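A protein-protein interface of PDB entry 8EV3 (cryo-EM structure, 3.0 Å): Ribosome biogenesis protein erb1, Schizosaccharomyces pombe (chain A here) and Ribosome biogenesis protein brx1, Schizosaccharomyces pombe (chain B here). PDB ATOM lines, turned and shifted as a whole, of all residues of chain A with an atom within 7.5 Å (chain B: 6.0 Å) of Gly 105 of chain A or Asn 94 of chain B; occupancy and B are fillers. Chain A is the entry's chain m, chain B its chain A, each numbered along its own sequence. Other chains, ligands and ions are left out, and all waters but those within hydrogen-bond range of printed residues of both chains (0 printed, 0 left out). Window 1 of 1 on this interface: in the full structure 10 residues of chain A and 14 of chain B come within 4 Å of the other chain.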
ATOM      1  N   GLU A 101      -1.935 -22.766 -27.877  1.00  0.00           N
ATOM      2  CA  GLU A 101      -1.097 -23.476 -26.919  1.00  0.00           C
ATOM      3  C   GLU A 101      -1.823 -23.668 -25.593  1.00  0.00           C
ATOM      4  O   GLU A 101      -2.767 -22.944 -25.283  1.00  0.00           O
ATOM      5  CB  GLU A 101       0.219 -22.726 -26.696  1.00  0.00           C
ATOM      6  CG  GLU A 101       0.053 -21.307 -26.168  1.00  0.00           C
ATOM      7  CD  GLU A 101       0.035 -21.240 -24.651  1.00  0.00           C
ATOM      8  OE1 GLU A 101       0.576 -22.164 -24.007  1.00  0.00           O
ATOM      9  OE2 GLU A 101      -0.520 -20.265 -24.104  1.00  0.00           O
ATOM     10  N   ILE A 102      -1.372 -24.648 -24.814  1.00  0.00           N
ATOM     11  CA  ILE A 102      -1.948 -24.918 -23.501  1.00  0.00           C
ATOM     12  C   ILE A 102      -0.828 -25.013 -22.476  1.00  0.00           C
ATOM     13  O   ILE A 102      -1.069 -25.332 -21.307  1.00  0.00           O
ATOM     14  CB  ILE A 102      -2.797 -26.202 -23.517  1.00  0.00           C
ATOM     15  CG1 ILE A 102      -2.001 -27.356 -24.123  1.00  0.00           C
ATOM     16  CG2 ILE A 102      -4.086 -25.980 -24.290  1.00  0.00           C
ATOM     17  CD1 ILE A 102      -2.742 -28.665 -24.114  1.00  0.00           C
ATOM     18  N   ASP A 103       0.407 -24.793 -22.930  1.00  0.00           N
ATOM     19  CA  ASP A 103       1.654 -24.698 -22.167  1.00  0.00           C
ATOM     20  C   ASP A 103       2.032 -25.992 -21.455  1.00  0.00           C
ATOM     21  O   ASP A 103       3.099 -26.041 -20.829  1.00  0.00           O
ATOM     22  CB  ASP A 103       1.657 -23.514 -21.176  1.00  0.00           C
ATOM     23  CG  ASP A 103       0.785 -23.731 -19.936  1.00  0.00           C
ATOM     24  OD1 ASP A 103       0.773 -24.829 -19.342  1.00  0.00           O
ATOM     25  OD2 ASP A 103       0.125 -22.756 -19.521  1.00  0.00           O
ATOM     26  N   ALA A 104       1.210 -27.040 -21.537  1.00  0.00           N
ATOM     27  CA  ALA A 104       1.531 -28.362 -20.988  1.00  0.00           C
ATOM     28  C   ALA A 104       1.972 -28.295 -19.527  1.00  0.00           C
ATOM     29  O   ALA A 104       2.742 -29.137 -19.059  1.00  0.00           O
ATOM     30  CB  ALA A 104       2.593 -29.063 -21.839  1.00  0.00           C
ATOM     31  N   GLY A 105       1.485 -27.300 -18.794  1.00  0.00           N
ATOM     32  CA  GLY A 105       1.844 -27.103 -17.409  1.00  0.00           C
ATOM     33  C   GLY A 105       0.939 -27.859 -16.459  1.00  0.00           C
ATOM     34  O   GLY A 105       0.214 -28.781 -16.845  1.00  0.00           O
ATOM     35  N   TYR A 106       1.001 -27.474 -15.187  1.00  0.00           N
ATOM     36  CA  TYR A 106       0.153 -28.046 -14.151  1.00  0.00           C
ATOM     37  C   TYR A 106      -0.609 -26.930 -13.453  1.00  0.00           C
ATOM     38  O   TYR A 106      -0.156 -25.784 -13.405  1.00  0.00           O
ATOM     39  CB  TYR A 106       0.954 -28.861 -13.112  1.00  0.00           C
ATOM     40  CG  TYR A 106       1.563 -30.159 -13.617  1.00  0.00           C
ATOM     41  CD1 TYR A 106       2.145 -30.252 -14.873  1.00  0.00           C
ATOM     42  CD2 TYR A 106       1.566 -31.291 -12.818  1.00  0.00           C
ATOM     43  CE1 TYR A 106       2.693 -31.436 -15.323  1.00  0.00           C
ATOM     44  CE2 TYR A 106       2.115 -32.477 -13.260  1.00  0.00           C
ATOM     45  CZ  TYR A 106       2.679 -32.543 -14.511  1.00  0.00           C
ATOM     46  OH  TYR A 106       3.228 -33.725 -14.952  1.00  0.00           O
ATOM     47  N   SER A 107      -1.781 -27.272 -12.917  1.00  0.00           N
ATOM     48  CA  SER A 107      -2.663 -26.303 -12.279  1.00  0.00           C
ATOM     49  C   SER A 107      -2.826 -26.568 -10.784  1.00  0.00           C
ATOM     50  O   SER A 107      -3.838 -26.189 -10.189  1.00  0.00           O
ATOM     51  CB  SER A 107      -4.026 -26.287 -12.968  1.00  0.00           C
ATOM     52  OG  SER A 107      -3.909 -25.881 -14.321  1.00  0.00           O
ATOM     53  N   SER A 108      -1.846 -27.231 -10.171  1.00  0.00           N
ATOM     54  CA  SER A 108      -1.772 -27.527  -8.742  1.00  0.00           C
ATOM     55  C   SER A 108      -2.880 -28.456  -8.264  1.00  0.00           C
ATOM     56  O   SER A 108      -2.938 -28.758  -7.065  1.00  0.00           O
ATOM     57  CB  SER A 108      -1.789 -26.257  -7.879  1.00  0.00           C
ATOM     58  OG  SER A 108      -2.307 -26.523  -6.587  1.00  0.00           O
ATOM     59  N   SER A 110      -3.766 -31.425 -10.310  1.00  0.00           N
ATOM     60  CA  SER A 110      -3.494 -32.750 -10.847  1.00  0.00           C
ATOM     61  C   SER A 110      -2.747 -33.593  -9.821  1.00  0.00           C
ATOM     62  O   SER A 110      -1.985 -33.074  -9.003  1.00  0.00           O
ATOM     63  CB  SER A 110      -2.684 -32.640 -12.140  1.00  0.00           C
ATOM     64  OG  SER A 110      -2.396 -33.920 -12.675  1.00  0.00           O
ATOM     65  N   ALA B  36      -3.054 -20.099 -16.516  1.00  0.00           N
ATOM     66  CA  ALA B  36      -3.008 -21.182 -17.492  1.00  0.00           C
ATOM     67  C   ALA B  36      -2.342 -22.424 -16.908  1.00  0.00           C
ATOM     68  O   ALA B  36      -2.818 -23.546 -17.109  1.00  0.00           O
ATOM     69  CB  ALA B  36      -2.281 -20.720 -18.754  1.00  0.00           C
ATOM     70  N   GLY B  37      -1.243 -22.245 -16.185  1.00  0.00           N
ATOM     71  CA  GLY B  37      -0.549 -23.378 -15.606  1.00  0.00           C
ATOM     72  C   GLY B  37       0.582 -22.935 -14.709  1.00  0.00           C
ATOM     73  O   GLY B  37       1.047 -21.792 -14.774  1.00  0.00           O
ATOM     74  N   PHE B  38       1.019 -23.865 -13.862  1.00  0.00           N
ATOM     75  CA  PHE B  38       2.140 -23.659 -12.959  1.00  0.00           C
ATOM     76  C   PHE B  38       3.073 -24.857 -13.049  1.00  0.00           C
ATOM     77  O   PHE B  38       2.632 -25.986 -13.282  1.00  0.00           O
ATOM     78  CB  PHE B  38       1.677 -23.464 -11.502  1.00  0.00           C
ATOM     79  CG  PHE B  38       0.651 -22.375 -11.322  1.00  0.00           C
ATOM     80  CD1 PHE B  38      -0.685 -22.599 -11.620  1.00  0.00           C
ATOM     81  CD2 PHE B  38       1.023 -21.130 -10.842  1.00  0.00           C
ATOM     82  CE1 PHE B  38      -1.626 -21.600 -11.452  1.00  0.00           C
ATOM     83  CE2 PHE B  38       0.084 -20.127 -10.670  1.00  0.00           C
ATOM     84  CZ  PHE B  38      -1.241 -20.364 -10.975  1.00  0.00           C
ATOM     85  N   VAL B  39       4.364 -24.602 -12.849  1.00  0.00           N
ATOM     86  CA  VAL B  39       5.412 -25.616 -12.978  1.00  0.00           C
ATOM     87  C   VAL B  39       5.292 -26.287 -14.342  1.00  0.00           C
ATOM     88  O   VAL B  39       4.947 -27.476 -14.417  1.00  0.00           O
ATOM     89  CB  VAL B  39       5.339 -26.650 -11.841  1.00  0.00           C
ATOM     90  CG1 VAL B  39       6.639 -27.434 -11.749  1.00  0.00           C
ATOM     91  CG2 VAL B  39       5.036 -25.966 -10.516  1.00  0.00           C
ATOM     92  N   PRO B  40       5.550 -25.578 -15.437  1.00  0.00           N
ATOM     93  CA  PRO B  40       5.317 -26.165 -16.761  1.00  0.00           C
ATOM     94  C   PRO B  40       6.300 -27.282 -17.074  1.00  0.00           C
ATOM     95  O   PRO B  40       7.490 -27.207 -16.762  1.00  0.00           O
ATOM     96  CB  PRO B  40       5.509 -24.979 -17.713  1.00  0.00           C
ATOM     97  CG  PRO B  40       6.420 -24.059 -16.978  1.00  0.00           C
ATOM     98  CD  PRO B  40       6.074 -24.204 -15.525  1.00  0.00           C
ATOM     99  N   ILE B  41       5.778 -28.324 -17.718  1.00  0.00           N
ATOM    100  CA  ILE B  41       6.567 -29.445 -18.219  1.00  0.00           C
ATOM    101  C   ILE B  41       6.499 -29.395 -19.735  1.00  0.00           C
ATOM    102  O   ILE B  41       5.464 -29.028 -20.303  1.00  0.00           O
ATOM    103  CB  ILE B  41       6.065 -30.810 -17.693  1.00  0.00           C
ATOM    104  CG1 ILE B  41       6.011 -30.863 -16.158  1.00  0.00           C
ATOM    105  CG2 ILE B  41       6.919 -31.956 -18.234  1.00  0.00           C
ATOM    106  CD1 ILE B  41       7.051 -30.036 -15.427  1.00  0.00           C
ATOM    107  N   LYS B  44       3.454 -33.292 -22.167  1.00  0.00           N
ATOM    108  CA  LYS B  44       2.479 -33.991 -21.339  1.00  0.00           C
ATOM    109  C   LYS B  44       1.492 -34.706 -22.250  1.00  0.00           C
ATOM    110  O   LYS B  44       0.864 -34.073 -23.103  1.00  0.00           O
ATOM    111  CB  LYS B  44       1.748 -33.025 -20.404  1.00  0.00           C
ATOM    112  CG  LYS B  44       1.117 -33.701 -19.199  1.00  0.00           C
ATOM    113  CD  LYS B  44       0.645 -32.688 -18.171  1.00  0.00           C
ATOM    114  CE  LYS B  44       0.051 -33.379 -16.955  1.00  0.00           C
ATOM    115  NZ  LYS B  44      -0.451 -32.398 -15.954  1.00  0.00           N
ATOM    116  N   LEU B  89     -10.620 -32.107 -23.459  1.00  0.00           N
ATOM    117  CA  LEU B  89     -10.050 -32.909 -22.384  1.00  0.00           C
ATOM    118  C   LEU B  89      -8.597 -32.538 -22.134  1.00  0.00           C
ATOM    119  O   LEU B  89      -8.155 -32.462 -20.982  1.00  0.00           O
ATOM    120  CB  LEU B  89     -10.163 -34.393 -22.721  1.00  0.00           C
ATOM    121  CG  LEU B  89     -11.242 -35.171 -21.981  1.00  0.00           C
ATOM    122  CD1 LEU B  89     -11.290 -36.599 -22.474  1.00  0.00           C
ATOM    123  CD2 LEU B  89     -10.984 -35.122 -20.490  1.00  0.00           C
ATOM    124  N   ALA B  90      -7.836 -32.314 -23.205  1.00  0.00           N
ATOM    125  CA  ALA B  90      -6.421 -31.999 -23.057  1.00  0.00           C
ATOM    126  C   ALA B  90      -6.220 -30.675 -22.334  1.00  0.00           C
ATOM    127  O   ALA B  90      -5.360 -30.566 -21.452  1.00  0.00           O
ATOM    128  CB  ALA B  90      -5.752 -31.972 -24.427  1.00  0.00           C
ATOM    129  N   GLU B  91      -7.003 -29.656 -22.692  1.00  0.00           N
ATOM    130  CA  GLU B  91      -6.905 -28.375 -22.002  1.00  0.00           C
ATOM    131  C   GLU B  91      -7.237 -28.527 -20.523  1.00  0.00           C
ATOM    132  O   GLU B  91      -6.637 -27.864 -19.671  1.00  0.00           O
ATOM    133  CB  GLU B  91      -7.831 -27.355 -22.668  1.00  0.00           C
ATOM    134  CG  GLU B  91      -8.174 -26.141 -21.813  1.00  0.00           C
ATOM    135  CD  GLU B  91      -9.434 -26.340 -20.989  1.00  0.00           C
ATOM    136  OE1 GLU B  91     -10.140 -27.344 -21.215  1.00  0.00           O
ATOM    137  OE2 GLU B  91      -9.717 -25.493 -20.116  1.00  0.00           O
ATOM    138  N   LEU B  92      -8.189 -29.405 -20.203  1.00  0.00           N
ATOM    139  CA  LEU B  92      -8.555 -29.636 -18.811  1.00  0.00           C
ATOM    140  C   LEU B  92      -7.373 -30.159 -18.006  1.00  0.00           C
ATOM    141  O   LEU B  92      -7.134 -29.716 -16.878  1.00  0.00           O
ATOM    142  CB  LEU B  92      -9.725 -30.615 -18.739  1.00  0.00           C
ATOM    143  CG  LEU B  92     -10.487 -30.694 -17.420  1.00  0.00           C
ATOM    144  CD1 LEU B  92     -11.381 -29.478 -17.252  1.00  0.00           C
ATOM    145  CD2 LEU B  92     -11.292 -31.981 -17.350  1.00  0.00           C
ATOM    146  N   TYR B  93      -6.621 -31.103 -18.569  1.00  0.00           N
ATOM    147  CA  TYR B  93      -5.468 -31.681 -17.897  1.00  0.00           C
ATOM    148  C   TYR B  93      -4.149 -31.060 -18.335  1.00  0.00           C
ATOM    149  O   TYR B  93      -3.092 -31.489 -17.858  1.00  0.00           O
ATOM    150  CB  TYR B  93      -5.428 -33.194 -18.130  1.00  0.00           C
ATOM    151  CG  TYR B  93      -6.513 -33.948 -17.402  1.00  0.00           C
ATOM    152  CD1 TYR B  93      -6.810 -33.666 -16.077  1.00  0.00           C
ATOM    153  CD2 TYR B  93      -7.240 -34.945 -18.037  1.00  0.00           C
ATOM    154  CE1 TYR B  93      -7.801 -34.352 -15.405  1.00  0.00           C
ATOM    155  CE2 TYR B  93      -8.233 -35.638 -17.373  1.00  0.00           C
ATOM    156  CZ  TYR B  93      -8.509 -35.337 -16.057  1.00  0.00           C
ATOM    157  OH  TYR B  93      -9.498 -36.023 -15.390  1.00  0.00           O
ATOM    158  N   ASN B  94      -4.184 -30.060 -19.220  1.00  0.00           N
ATOM    159  CA  ASN B  94      -2.982 -29.374 -19.699  1.00  0.00           C
ATOM    160  C   ASN B  94      -1.969 -30.361 -20.281  1.00  0.00           C
ATOM    161  O   ASN B  94      -0.780 -30.331 -19.960  1.00  0.00           O
ATOM    162  CB  ASN B  94      -2.353 -28.531 -18.587  1.00  0.00           C
ATOM    163  CG  ASN B  94      -3.119 -27.252 -18.324  1.00  0.00           C
ATOM    164  OD1 ASN B  94      -3.998 -26.873 -19.095  1.00  0.00           O
ATOM    165  ND2 ASN B  94      -2.791 -26.582 -17.227  1.00  0.00           N
ATOM    166  N   CYS B  95      -2.456 -31.252 -21.139  1.00  0.00           N
ATOM    167  CA  CYS B  95      -1.620 -32.223 -21.834  1.00  0.00           C
ATOM    168  C   CYS B  95      -1.588 -31.858 -23.310  1.00  0.00           C
ATOM    169  O   CYS B  95      -2.634 -31.829 -23.966  1.00  0.00           O
ATOM    170  CB  CYS B  95      -2.153 -33.642 -21.643  1.00  0.00           C
ATOM    171  SG  CYS B  95      -2.371 -34.137 -19.921  1.00  0.00           S
ATOM    172  N   ASN B  96      -0.393 -31.585 -23.836  1.00  0.00           N
ATOM    173  CA  ASN B  96      -0.270 -31.171 -25.228  1.00  0.00           C
ATOM    174  C   ASN B  96      -0.287 -32.339 -26.206  1.00  0.00           C
ATOM    175  O   ASN B  96      -0.431 -32.110 -27.410  1.00  0.00           O
ATOM    176  CB  ASN B  96       1.004 -30.345 -25.425  1.00  0.00           C
ATOM    177  CG  ASN B  96       2.252 -31.069 -24.962  1.00  0.00           C
ATOM    178  OD1 ASN B  96       2.209 -32.245 -24.608  1.00  0.00           O
ATOM    179  ND2 ASN B  96       3.376 -30.363 -24.958  1.00  0.00           N
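The backbone carbonyl oxygen (O) of Ala 36 of chain B sits at hydrogen-bond distance from the side-chain amide nitrogen (ND2) of Asn 94 of chain B, 3.0 Å away.
OE1 of Glu 101 of chain A sits at hydrogen-bond distance from N of Asp 103 of chain A.
The side-chain carboxylate (OD1) of Asp 103 of chain A lies within hydrogen-bond range of the backbone NH (N) of Gly 105 of chain A (2.6 Å).
The backbone carbonyl oxygen of Lys 44 of chain B sits close to the side-chain amide oxygen of Asn 96 of chain B, 2.7 Å away.
The side-chain amide oxygen of Asn 94 of chain B lies close to the backbone carbonyl oxygen of Glu 91 of chain B, at 2.9 Å.
O of Ala 90 of chain B lies within hydrogen-bond range of N of Cys 95 of chain B, at 3.0 Å.
Of the 9 printed residues of chain A, 6 touch a printed residue of chain B.
Printed residues of chain A that touch a printed residue of chain B: Ile 102, Asp 103, Ala 104, Gly 105, Tyr 106 and Ser 107.
Printed residues of chain B that touch a printed residue of chain A: Ala 36, Gly 37, Phe 38, Val 39, Pro 40, Ile 41, Lys 44, Asn 94, Cys 95 and Asn 96.
Along chain B the printed residues that touch a printed residue of chain A span positions 36 to 96.
Among the printed residues, no Asp or Glu carboxylate lies within 4 Å of a Lys or Arg side-chain nitrogen of the other chain.
The backbone NH (N) of Tyr 106 of chain A lies within hydrogen-bond range of the backbone carbonyl oxygen (O) of Phe 38 of chain B.
The side-chain hydroxyl of Ser 107 of chain A sits at hydrogen-bond distance from the side-chain amide nitrogen of Asn 94 of chain B, at 3.2 Å.
N of Ile 41 of chain B lies within hydrogen-bond range of O of Ala 104 of chain A, 3.4 Å away.
Printed residues of chain B within 4 Å of Ile 102 of chain A: Asn 94 (3.98 Å), Cys 95 (3.2 Å) and Asn 96 (3.7 Å).
Of the printed residues of chain B, Gly 105 of chain A touches Pro 40, Lys 44 and Asn 94.
Of the printed residues of chain B, Tyr 106 of chain A touches Gly 37, Phe 38, Val 39, Ile 41 and Lys 44.
Printed residues of chain A within 4 Å of Gly 37 of chain B: Asp 103 and Tyr 106.
Of the printed residues of chain A, Ile 41 of chain B touches Asp 103 (3.8 Å), Ala 104 (3.0 Å) and Tyr 106 (3.5 Å).
Leu 89 of chain B touches none of the printed residues of chain A.
Tyr 93 of chain B touches none of the printed residues of chain A.
Of the printed residues of chain A, Asn 94 of chain B touches Ile 102 (3.98 Å), Ala 104 (3.2 Å), Gly 105 (3.1 Å) and Ser 107 (3.2 Å).
Among the printed residues, pairs that only touch across the chains: Gly 105 of chain A with Asn 94 of chain B (3.1 Å), Ile 102 of chain A with Cys 95 of chain B (3.2 Å), Ala 104 of chain A with Asn 94 of chain B (3.2 Å), Tyr 106 of chain A with Gly 37 of chain B (3.2 Å), Asp 103 of chain A with Ala 36 of chain B (3.2 Å), Tyr 106 of chain A with Lys 44 of chain B (3.3 Å), Ala 104 of chain A with Asn 96 of chain B (3.5 Å), Tyr 106 of chain A with Ile 41 of chain B (3.5 Å), Asp 103 of chain A with Gly 37 of chain B (3.6 Å), Gly 105 of chain A with Pro 40 of chain B (3.7 Å), Ile 102 of chain A with Asn 96 of chain B (3.7 Å), Gly 105 of chain A with Lys 44 of chain B (3.8 Å), Ser 107 of chain A with Ala 36 of chain B (3.8 Å), Asp 103 of chain A with Ile 41 of chain B (3.8 Å), Tyr 106 of chain A with Val 39 of chain B (3.97 Å) and Ile 102 of chain A with Asn 94 of chain B (3.98 Å).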
